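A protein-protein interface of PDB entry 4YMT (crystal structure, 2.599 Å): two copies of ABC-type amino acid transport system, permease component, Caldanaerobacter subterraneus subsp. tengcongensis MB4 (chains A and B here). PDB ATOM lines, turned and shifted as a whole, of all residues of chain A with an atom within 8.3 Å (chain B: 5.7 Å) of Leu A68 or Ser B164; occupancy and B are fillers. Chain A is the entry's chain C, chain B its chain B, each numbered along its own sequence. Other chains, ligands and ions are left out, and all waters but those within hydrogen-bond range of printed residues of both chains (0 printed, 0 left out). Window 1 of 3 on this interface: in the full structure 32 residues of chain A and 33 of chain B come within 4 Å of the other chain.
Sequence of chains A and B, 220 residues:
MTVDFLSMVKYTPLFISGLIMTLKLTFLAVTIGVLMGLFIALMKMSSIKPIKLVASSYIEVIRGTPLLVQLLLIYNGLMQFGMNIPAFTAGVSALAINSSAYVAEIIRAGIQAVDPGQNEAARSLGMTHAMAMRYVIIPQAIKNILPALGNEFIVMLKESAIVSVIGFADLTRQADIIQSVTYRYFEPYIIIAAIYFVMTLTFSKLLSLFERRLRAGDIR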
ATOM      1  N   THR A  65       5.848  -2.884   5.181  1.00  0.00           N
ATOM      2  CA  THR A  65       5.463  -3.757   4.080  1.00  0.00           C
ATOM      3  C   THR A  65       3.956  -4.093   4.147  1.00  0.00           C
ATOM      4  O   THR A  65       3.389  -4.168   5.241  1.00  0.00           O
ATOM      5  CB  THR A  65       6.360  -5.015   4.114  1.00  0.00           C
ATOM      6  OG1 THR A  65       6.782  -5.335   2.783  1.00  0.00           O
ATOM      7  CG2 THR A  65       5.676  -6.197   4.802  1.00  0.00           C
ATOM      8  N   PRO A  66       3.299  -4.277   2.974  1.00  0.00           N
ATOM      9  CA  PRO A  66       1.829  -4.399   2.898  1.00  0.00           C
ATOM     10  C   PRO A  66       1.254  -5.607   3.619  1.00  0.00           C
ATOM     11  O   PRO A  66       1.911  -6.639   3.655  1.00  0.00           O
ATOM     12  CB  PRO A  66       1.563  -4.520   1.395  1.00  0.00           C
ATOM     13  CG  PRO A  66       2.754  -3.933   0.728  1.00  0.00           C
ATOM     14  CD  PRO A  66       3.907  -4.314   1.632  1.00  0.00           C
ATOM     15  N   LEU A  67       0.064  -5.468   4.206  1.00  0.00           N
ATOM     16  CA  LEU A  67      -0.625  -6.585   4.861  1.00  0.00           C
ATOM     17  C   LEU A  67      -0.967  -7.696   3.837  1.00  0.00           C
ATOM     18  O   LEU A  67      -0.876  -8.893   4.145  1.00  0.00           O
ATOM     19  CB  LEU A  67      -1.900  -6.090   5.545  1.00  0.00           C
ATOM     20  CG  LEU A  67      -2.515  -6.790   6.771  1.00  0.00           C
ATOM     21  CD1 LEU A  67      -4.022  -6.670   6.697  1.00  0.00           C
ATOM     22  CD2 LEU A  67      -2.108  -8.236   6.975  1.00  0.00           C
ATOM     23  N   LEU A  68      -1.386  -7.275   2.639  1.00  0.00           N
ATOM     24  CA  LEU A  68      -1.776  -8.174   1.555  1.00  0.00           C
ATOM     25  C   LEU A  68      -0.664  -9.167   1.248  1.00  0.00           C
ATOM     26  O   LEU A  68      -0.883 -10.387   1.268  1.00  0.00           O
ATOM     27  CB  LEU A  68      -2.123  -7.384   0.289  1.00  0.00           C
ATOM     28  CG  LEU A  68      -3.289  -7.909  -0.567  1.00  0.00           C
ATOM     29  CD1 LEU A  68      -3.160  -7.526  -2.049  1.00  0.00           C
ATOM     30  CD2 LEU A  68      -3.496  -9.409  -0.423  1.00  0.00           C
ATOM     31  N   VAL A  69       0.519  -8.630   0.950  1.00  0.00           N
ATOM     32  CA  VAL A  69       1.682  -9.447   0.637  1.00  0.00           C
ATOM     33  C   VAL A  69       2.000 -10.430   1.754  1.00  0.00           C
ATOM     34  O   VAL A  69       2.449 -11.532   1.477  1.00  0.00           O
ATOM     35  CB  VAL A  69       2.912  -8.582   0.349  1.00  0.00           C
ATOM     36  CG1 VAL A  69       4.141  -9.443   0.103  1.00  0.00           C
ATOM     37  CG2 VAL A  69       2.636  -7.644  -0.822  1.00  0.00           C
ATOM     38  N   GLN A  70       1.726 -10.059   3.004  1.00  0.00           N
ATOM     39  CA  GLN A  70       1.966 -10.961   4.139  1.00  0.00           C
ATOM     40  C   GLN A  70       0.945 -12.105   4.141  1.00  0.00           C
ATOM     41  O   GLN A  70       1.297 -13.275   4.400  1.00  0.00           O
ATOM     42  CB  GLN A  70       1.927 -10.189   5.468  1.00  0.00           C
ATOM     43  CG  GLN A  70       3.039  -9.160   5.598  1.00  0.00           C
ATOM     44  CD  GLN A  70       2.859  -8.172   6.763  1.00  0.00           C
ATOM     45  OE1 GLN A  70       3.378  -7.059   6.716  1.00  0.00           O
ATOM     46  NE2 GLN A  70       2.163  -8.597   7.821  1.00  0.00           N
ATOM     47  N   LEU A  71      -0.309 -11.754   3.848  1.00  0.00           N
ATOM     48  CA  LEU A  71      -1.399 -12.726   3.717  1.00  0.00           C
ATOM     49  C   LEU A  71      -1.079 -13.756   2.636  1.00  0.00           C
ATOM     50  O   LEU A  71      -1.005 -14.954   2.906  1.00  0.00           O
ATOM     51  CB  LEU A  71      -2.717 -12.022   3.360  1.00  0.00           C
ATOM     52  CG  LEU A  71      -4.032 -12.484   4.002  1.00  0.00           C
ATOM     53  CD1 LEU A  71      -5.190 -12.335   3.030  1.00  0.00           C
ATOM     54  CD2 LEU A  71      -3.946 -13.894   4.561  1.00  0.00           C
ATOM     55  N   LEU A  72      -0.882 -13.267   1.413  1.00  0.00           N
ATOM     56  CA  LEU A  72      -0.594 -14.120   0.274  1.00  0.00           C
ATOM     57  C   LEU A  72       0.679 -14.924   0.492  1.00  0.00           C
ATOM     58  O   LEU A  72       0.739 -16.091   0.129  1.00  0.00           O
ATOM     59  CB  LEU A  72      -0.502 -13.293  -1.007  1.00  0.00           C
ATOM     60  CG  LEU A  72      -1.758 -12.480  -1.346  1.00  0.00           C
ATOM     61  CD1 LEU A  72      -1.634 -11.753  -2.683  1.00  0.00           C
ATOM     62  CD2 LEU A  72      -2.999 -13.354  -1.332  1.00  0.00           C
ATOM     63  N   LEU A  73       1.693 -14.305   1.085  1.00  0.00           N
ATOM     64  CA  LEU A  73       2.923 -15.021   1.412  1.00  0.00           C
ATOM     65  C   LEU A  73       2.641 -16.198   2.342  1.00  0.00           C
ATOM     66  O   LEU A  73       3.292 -17.234   2.235  1.00  0.00           O
ATOM     67  CB  LEU A  73       3.950 -14.089   2.060  1.00  0.00           C
ATOM     68  CG  LEU A  73       5.300 -14.719   2.382  1.00  0.00           C
ATOM     69  CD1 LEU A  73       5.857 -15.415   1.151  1.00  0.00           C
ATOM     70  CD2 LEU A  73       6.243 -13.654   2.845  1.00  0.00           C
ATOM     71  N   ILE A  74       1.687 -16.050   3.261  1.00  0.00           N
ATOM     72  CA  ILE A  74       1.323 -17.196   4.102  1.00  0.00           C
ATOM     73  C   ILE A  74       0.477 -18.244   3.350  1.00  0.00           C
ATOM     74  O   ILE A  74       0.789 -19.432   3.361  1.00  0.00           O
ATOM     75  CB  ILE A  74       0.558 -16.758   5.359  1.00  0.00           C
ATOM     76  CG1 ILE A  74       1.452 -15.902   6.254  1.00  0.00           C
ATOM     77  CG2 ILE A  74       0.085 -17.967   6.137  1.00  0.00           C
ATOM     78  CD1 ILE A  74       0.876 -15.694   7.636  1.00  0.00           C
ATOM     79  N   TYR A  75      -0.570 -17.788   2.669  1.00  0.00           N
ATOM     80  CA  TYR A  75      -1.547 -18.671   2.041  1.00  0.00           C
ATOM     81  C   TYR A  75      -1.008 -19.354   0.782  1.00  0.00           C
ATOM     82  O   TYR A  75      -1.134 -20.563   0.624  1.00  0.00           O
ATOM     83  CB  TYR A  75      -2.807 -17.873   1.693  1.00  0.00           C
ATOM     84  CG  TYR A  75      -3.994 -18.691   1.208  1.00  0.00           C
ATOM     85  CD1 TYR A  75      -4.384 -18.646  -0.123  1.00  0.00           C
ATOM     86  CD2 TYR A  75      -4.721 -19.500   2.077  1.00  0.00           C
ATOM     87  CE1 TYR A  75      -5.458 -19.378  -0.581  1.00  0.00           C
ATOM     88  CE2 TYR A  75      -5.803 -20.232   1.628  1.00  0.00           C
ATOM     89  CZ  TYR A  75      -6.163 -20.169   0.293  1.00  0.00           C
ATOM     90  OH  TYR A  75      -7.232 -20.891  -0.180  1.00  0.00           O
ATOM     91  N   ASN A  76      -0.391 -18.573  -0.098  1.00  0.00           N
ATOM     92  CA  ASN A  76       0.099 -19.067  -1.379  1.00  0.00           C
ATOM     93  C   ASN A  76       1.557 -19.509  -1.365  1.00  0.00           C
ATOM     94  O   ASN A  76       1.916 -20.538  -1.946  1.00  0.00           O
ATOM     95  CB  ASN A  76      -0.077 -17.986  -2.439  1.00  0.00           C
ATOM     96  CG  ASN A  76      -1.526 -17.711  -2.745  1.00  0.00           C
ATOM     97  OD1 ASN A  76      -2.407 -18.482  -2.364  1.00  0.00           O
ATOM     98  ND2 ASN A  76      -1.786 -16.611  -3.442  1.00  0.00           N
ATOM     99  N   ALA A  94      -1.959 -13.836   9.507  1.00  0.00           N
ATOM    100  CA  ALA A  94      -1.475 -12.634   8.838  1.00  0.00           C
ATOM    101  C   ALA A  94      -1.841 -11.390   9.649  1.00  0.00           C
ATOM    102  O   ALA A  94      -0.976 -10.547   9.943  1.00  0.00           O
ATOM    103  CB  ALA A  94      -2.041 -12.541   7.439  1.00  0.00           C
ATOM    104  N   LEU A  95      -3.106 -11.318  10.060  1.00  0.00           N
ATOM    105  CA  LEU A  95      -3.603 -10.162  10.793  1.00  0.00           C
ATOM    106  C   LEU A  95      -2.945 -10.023  12.174  1.00  0.00           C
ATOM    107  O   LEU A  95      -2.553  -8.923  12.537  1.00  0.00           O
ATOM    108  CB  LEU A  95      -5.132 -10.221  10.935  1.00  0.00           C
ATOM    109  CG  LEU A  95      -6.024 -10.006   9.697  1.00  0.00           C
ATOM    110  CD1 LEU A  95      -7.484  -9.873  10.108  1.00  0.00           C
ATOM    111  CD2 LEU A  95      -5.614  -8.815   8.837  1.00  0.00           C
ATOM    112  N   ASN A  98       0.675  -8.844  11.737  1.00  0.00           N
ATOM    113  CA  ASN A  98       0.696  -7.423  11.404  1.00  0.00           C
ATOM    114  C   ASN A  98       0.427  -6.560  12.668  1.00  0.00           C
ATOM    115  O   ASN A  98       1.150  -5.572  13.011  1.00  0.00           O
ATOM    116  CB  ASN A  98      -0.333  -7.191  10.311  1.00  0.00           C
ATOM    117  CG  ASN A  98      -0.252  -5.828   9.701  1.00  0.00           C
ATOM    118  OD1 ASN A  98      -1.109  -4.990   9.935  1.00  0.00           O
ATOM    119  ND2 ASN A  98       0.770  -5.599   8.893  1.00  0.00           N
ATOM    120  N   GLU A 159      -9.292  -3.467   8.145  1.00  0.00           N
ATOM    121  CA  GLU A 159      -8.207  -4.224   7.535  1.00  0.00           C
ATOM    122  C   GLU A 159      -8.596  -5.670   7.210  1.00  0.00           C
ATOM    123  O   GLU A 159      -8.174  -6.201   6.185  1.00  0.00           O
ATOM    124  CB  GLU A 159      -6.980  -4.207   8.462  1.00  0.00           C
ATOM    125  CG  GLU A 159      -6.325  -2.843   8.558  1.00  0.00           C
ATOM    126  CD  GLU A 159      -5.482  -2.523   7.338  1.00  0.00           C
ATOM    127  OE1 GLU A 159      -4.835  -3.455   6.821  1.00  0.00           O
ATOM    128  OE2 GLU A 159      -5.476  -1.368   6.870  1.00  0.00           O
ATOM    129  N   ILE A 162      -9.605  -7.752   3.953  1.00  0.00           N
ATOM    130  CA  ILE A 162      -8.643  -8.161   2.934  1.00  0.00           C
ATOM    131  C   ILE A 162      -8.613  -9.675   2.770  1.00  0.00           C
ATOM    132  O   ILE A 162      -8.142 -10.172   1.756  1.00  0.00           O
ATOM    133  CB  ILE A 162      -7.215  -7.661   3.266  1.00  0.00           C
ATOM    134  CG1 ILE A 162      -6.337  -7.672   2.015  1.00  0.00           C
ATOM    135  CG2 ILE A 162      -6.581  -8.517   4.342  1.00  0.00           C
ATOM    136  CD1 ILE A 162      -6.886  -6.833   0.897  1.00  0.00           C
ATOM    137  N   VAL A 163      -9.140 -10.404   3.752  1.00  0.00           N
ATOM    138  CA  VAL A 163      -9.140 -11.860   3.705  1.00  0.00           C
ATOM    139  C   VAL A 163     -10.278 -12.342   2.804  1.00  0.00           C
ATOM    140  O   VAL A 163     -10.504 -13.544   2.638  1.00  0.00           O
ATOM    141  CB  VAL A 163      -9.278 -12.480   5.099  1.00  0.00           C
ATOM    142  CG1 VAL A 163      -8.269 -11.876   6.024  1.00  0.00           C
ATOM    143  CG2 VAL A 163     -10.678 -12.270   5.624  1.00  0.00           C
ATOM    144  N   SER A 164     -11.013 -11.384   2.256  1.00  0.00           N
ATOM    145  CA  SER A 164     -12.004 -11.665   1.255  1.00  0.00           C
ATOM    146  C   SER A 164     -11.323 -12.302   0.083  1.00  0.00           C
ATOM    147  O   SER A 164     -11.775 -13.327  -0.424  1.00  0.00           O
ATOM    148  CB  SER A 164     -12.683 -10.383   0.789  1.00  0.00           C
ATOM    149  OG  SER A 164     -13.983 -10.285   1.309  1.00  0.00           O
ATOM    150  N   VAL A 165     -10.195 -11.721  -0.318  1.00  0.00           N
ATOM    151  CA  VAL A 165      -9.540 -12.126  -1.558  1.00  0.00           C
ATOM    152  C   VAL A 165      -9.031 -13.561  -1.494  1.00  0.00           C
ATOM    153  O   VAL A 165      -8.704 -14.170  -2.512  1.00  0.00           O
ATOM    154  CB  VAL A 165      -8.363 -11.196  -1.887  1.00  0.00           C
ATOM    155  CG1 VAL A 165      -8.751  -9.753  -1.635  1.00  0.00           C
ATOM    156  CG2 VAL A 165      -7.142 -11.587  -1.066  1.00  0.00           C
ATOM    157  N   ILE A 166      -9.005 -14.092  -0.281  1.00  0.00           N
ATOM    158  CA  ILE A 166      -8.474 -15.408   0.008  1.00  0.00           C
ATOM    159  C   ILE A 166      -9.650 -16.387   0.066  1.00  0.00           C
ATOM    160  O   ILE A 166      -9.474 -17.594   0.208  1.00  0.00           O
ATOM    161  CB  ILE A 166      -7.669 -15.366   1.341  1.00  0.00           C
ATOM    162  CG1 ILE A 166      -6.384 -16.161   1.254  1.00  0.00           C
ATOM    163  CG2 ILE A 166      -8.488 -15.829   2.538  1.00  0.00           C
ATOM    164  CD1 ILE A 166      -5.708 -16.222   2.590  1.00  0.00           C
ATOM    165  N   SER B 160      -1.653   0.586  -2.183  1.00  0.00           N
ATOM    166  CA  SER B 160      -1.911   0.382  -3.609  1.00  0.00           C
ATOM    167  C   SER B 160      -1.832  -1.095  -4.024  1.00  0.00           C
ATOM    168  O   SER B 160      -2.398  -1.491  -5.041  1.00  0.00           O
ATOM    169  CB  SER B 160      -0.942   1.216  -4.451  1.00  0.00           C
ATOM    170  OG  SER B 160       0.374   0.705  -4.354  1.00  0.00           O
ATOM    171  N   ALA B 161      -1.149  -1.912  -3.232  1.00  0.00           N
ATOM    172  CA  ALA B 161      -1.048  -3.341  -3.525  1.00  0.00           C
ATOM    173  C   ALA B 161      -2.429  -4.013  -3.643  1.00  0.00           C
ATOM    174  O   ALA B 161      -2.540  -5.148  -4.101  1.00  0.00           O
ATOM    175  CB  ALA B 161      -0.208  -4.044  -2.455  1.00  0.00           C
ATOM    176  N   ILE B 162      -3.478  -3.315  -3.224  1.00  0.00           N
ATOM    177  CA  ILE B 162      -4.799  -3.913  -3.160  1.00  0.00           C
ATOM    178  C   ILE B 162      -5.444  -4.001  -4.529  1.00  0.00           C
ATOM    179  O   ILE B 162      -6.448  -4.678  -4.697  1.00  0.00           O
ATOM    180  CB  ILE B 162      -5.732  -3.133  -2.234  1.00  0.00           C
ATOM    181  CG1 ILE B 162      -6.787  -4.070  -1.656  1.00  0.00           C
ATOM    182  CG2 ILE B 162      -6.306  -1.889  -2.938  1.00  0.00           C
ATOM    183  CD1 ILE B 162      -7.731  -3.365  -0.770  1.00  0.00           C
ATOM    184  N   VAL B 163      -4.898  -3.278  -5.498  1.00  0.00           N
ATOM    185  CA  VAL B 163      -5.446  -3.308  -6.842  1.00  0.00           C
ATOM    186  C   VAL B 163      -4.955  -4.548  -7.598  1.00  0.00           C
ATOM    187  O   VAL B 163      -5.337  -4.783  -8.749  1.00  0.00           O
ATOM    188  CB  VAL B 163      -5.056  -2.052  -7.620  1.00  0.00           C
ATOM    189  CG1 VAL B 163      -5.362  -0.812  -6.784  1.00  0.00           C
ATOM    190  CG2 VAL B 163      -3.576  -2.109  -7.967  1.00  0.00           C
ATOM    191  N   SER B 164      -4.103  -5.337  -6.950  1.00  0.00           N
ATOM    192  CA  SER B 164      -3.691  -6.604  -7.519  1.00  0.00           C
ATOM    193  C   SER B 164      -4.933  -7.479  -7.677  1.00  0.00           C
ATOM    194  O   SER B 164      -5.130  -8.094  -8.729  1.00  0.00           O
ATOM    195  CB  SER B 164      -2.629  -7.289  -6.655  1.00  0.00           C
ATOM    196  OG  SER B 164      -3.212  -8.204  -5.750  1.00  0.00           O
ATOM    197  N   VAL B 165      -5.795  -7.484  -6.659  1.00  0.00           N
ATOM    198  CA  VAL B 165      -6.958  -8.378  -6.637  1.00  0.00           C
ATOM    199  C   VAL B 165      -7.967  -8.084  -7.754  1.00  0.00           C
ATOM    200  O   VAL B 165      -8.867  -8.879  -8.020  1.00  0.00           O
ATOM    201  CB  VAL B 165      -7.688  -8.311  -5.279  1.00  0.00           C
ATOM    202  CG1 VAL B 165      -6.692  -8.329  -4.146  1.00  0.00           C
ATOM    203  CG2 VAL B 165      -8.568  -7.094  -5.207  1.00  0.00           C
ATOM    204  N   ILE B 166      -7.784  -6.948  -8.411  1.00  0.00           N
ATOM    205  CA  ILE B 166      -8.673  -6.445  -9.452  1.00  0.00           C
ATOM    206  C   ILE B 166      -8.082  -6.860 -10.804  1.00  0.00           C
ATOM    207  O   ILE B 166      -8.672  -6.657 -11.884  1.00  0.00           O
ATOM    208  CB  ILE B 166      -8.797  -4.901  -9.336  1.00  0.00           C
ATOM    209  CG1 ILE B 166     -10.216  -4.409  -9.528  1.00  0.00           C
ATOM    210  CG2 ILE B 166      -7.860  -4.167 -10.289  1.00  0.00           C
ATOM    211  CD1 ILE B 166     -10.257  -2.889  -9.577  1.00  0.00           C
ATOM    212  N   GLY B 167      -6.876  -7.414 -10.723  1.00  0.00           N
ATOM    213  CA  GLY B 167      -6.168  -7.860 -11.899  1.00  0.00           C
ATOM    214  C   GLY B 167      -5.303  -6.779 -12.514  1.00  0.00           C
ATOM    215  O   GLY B 167      -4.950  -6.870 -13.691  1.00  0.00           O
ATOM    216  N   PHE B 168      -4.993  -5.732 -11.749  1.00  0.00           N
ATOM    217  CA  PHE B 168      -4.059  -4.710 -12.224  1.00  0.00           C
ATOM    218  C   PHE B 168      -2.623  -5.190 -12.024  1.00  0.00           C
ATOM    219  O   PHE B 168      -2.306  -5.806 -11.000  1.00  0.00           O
ATOM    220  CB  PHE B 168      -4.278  -3.383 -11.510  1.00  0.00           C
ATOM    221  CG  PHE B 168      -3.366  -2.295 -11.986  1.00  0.00           C
ATOM    222  CD1 PHE B 168      -3.530  -1.746 -13.247  1.00  0.00           C
ATOM    223  CD2 PHE B 168      -2.328  -1.840 -11.187  1.00  0.00           C
ATOM    224  CE1 PHE B 168      -2.681  -0.757 -13.699  1.00  0.00           C
ATOM    225  CE2 PHE B 168      -1.475  -0.845 -11.630  1.00  0.00           C
ATOM    226  CZ  PHE B 168      -1.653  -0.303 -12.886  1.00  0.00           C
ATOM    227  N   ASP B 170       0.267  -4.502 -10.822  1.00  0.00           N
ATOM    228  CA  ASP B 170       1.141  -3.777  -9.905  1.00  0.00           C
ATOM    229  C   ASP B 170       2.306  -4.675  -9.491  1.00  0.00           C
ATOM    230  O   ASP B 170       2.565  -5.690 -10.134  1.00  0.00           O
ATOM    231  CB  ASP B 170       0.366  -3.307  -8.671  1.00  0.00           C
ATOM    232  CG  ASP B 170       0.103  -4.435  -7.678  1.00  0.00           C
ATOM    233  OD1 ASP B 170      -0.050  -5.601  -8.104  1.00  0.00           O
ATOM    234  OD2 ASP B 170       0.055  -4.162  -6.461  1.00  0.00           O
ATOM    235  N   THR B 172       2.520  -6.436  -6.673  1.00  0.00           N
ATOM    236  CA  THR B 172       2.049  -7.632  -5.974  1.00  0.00           C
ATOM    237  C   THR B 172       1.514  -8.669  -6.974  1.00  0.00           C
ATOM    238  O   THR B 172       1.627  -9.884  -6.757  1.00  0.00           O
ATOM    239  CB  THR B 172       0.960  -7.279  -4.929  1.00  0.00           C
ATOM    240  OG1 THR B 172       1.481  -6.317  -4.008  1.00  0.00           O
ATOM    241  CG2 THR B 172       0.545  -8.504  -4.140  1.00  0.00           C
ATOM    242  N   ARG B 173       0.926  -8.177  -8.061  1.00  0.00           N
ATOM    243  CA  ARG B 173       0.370  -9.028  -9.105  1.00  0.00           C
ATOM    244  C   ARG B 173       1.444  -9.888  -9.776  1.00  0.00           C
ATOM    245  O   ARG B 173       1.166 -11.007 -10.212  1.00  0.00           O
ATOM    246  CB  ARG B 173      -0.343  -8.159 -10.145  1.00  0.00           C
ATOM    247  CG  ARG B 173      -1.009  -8.880 -11.318  1.00  0.00           C
ATOM    248  CD  ARG B 173      -2.078  -9.891 -10.901  1.00  0.00           C
ATOM    249  NE  ARG B 173      -3.112 -10.030 -11.936  1.00  0.00           N
ATOM    250  CZ  ARG B 173      -2.944 -10.650 -13.108  1.00  0.00           C
ATOM    251  NH1 ARG B 173      -1.775 -11.193 -13.428  1.00  0.00           N
ATOM    252  NH2 ARG B 173      -3.947 -10.725 -13.976  1.00  0.00           N
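OD1 of Asp B170 sits at hydrogen-bond distance from N of Thr B172, 3.1 Å away.
Of the 12 printed residues of chain B, 5 touch a printed residue of chain A.
Hydrophobic or aromatic side chains of chain B within 4 Å of the printed part of chain A: Ile B162 and Val B165.
Of the 21 printed residues of chain A, 4 touch a printed residue of chain B.
Printed residues of chain A that touch a printed residue of chain B: Leu A68, Val A69, Ile A162 and Val A165.
Hydrophobic or aromatic side chains of chain A that line the printed part of chain B: Leu A68, Val A69, Ile A162 and Val A165.
Among the printed residues, 5 pairs touch across the chains.
Among the printed residues, no Asp or Glu carboxylate lies within 4 Å of a Lys or Arg side-chain nitrogen of the other chain.
Among the printed residues, pairs that only touch across the chains: Leu A68 with Ala B161, Leu A68 with Ser B164, Val A69 with Thr B172, Ile A162 with Ile B162 and Val A165 with Val B165.
Printed residues of chain B within 4 Å of Leu A68: Ala B161 and Ser B164.
Tyr A75 touches none of the printed residues of chain B.
Printed residues of chain B within 4 Å of Ile A162: Ile B162 (3.8 Å).
Of the printed residues of chain A, Ala B161 touches Leu A68.
Printed residues of chain A within 4 Å of Ser B164: Leu A68.
Asp B170 touches none of the printed residues of chain A.
Printed residues of chain A within 4 Å of Thr B172: Val A69.
The nearest residue of chain B that does not touch Leu A68 is Ile B162 (4.1 Å).
The nearest residue of chain A that does not touch Ser B164 is Leu A72 (4.9 Å).
Ile A162 touches its own counterpart, Ile B162.
Val A165 touches its own counterpart, Val B165.
5 positions are printed for both chains.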
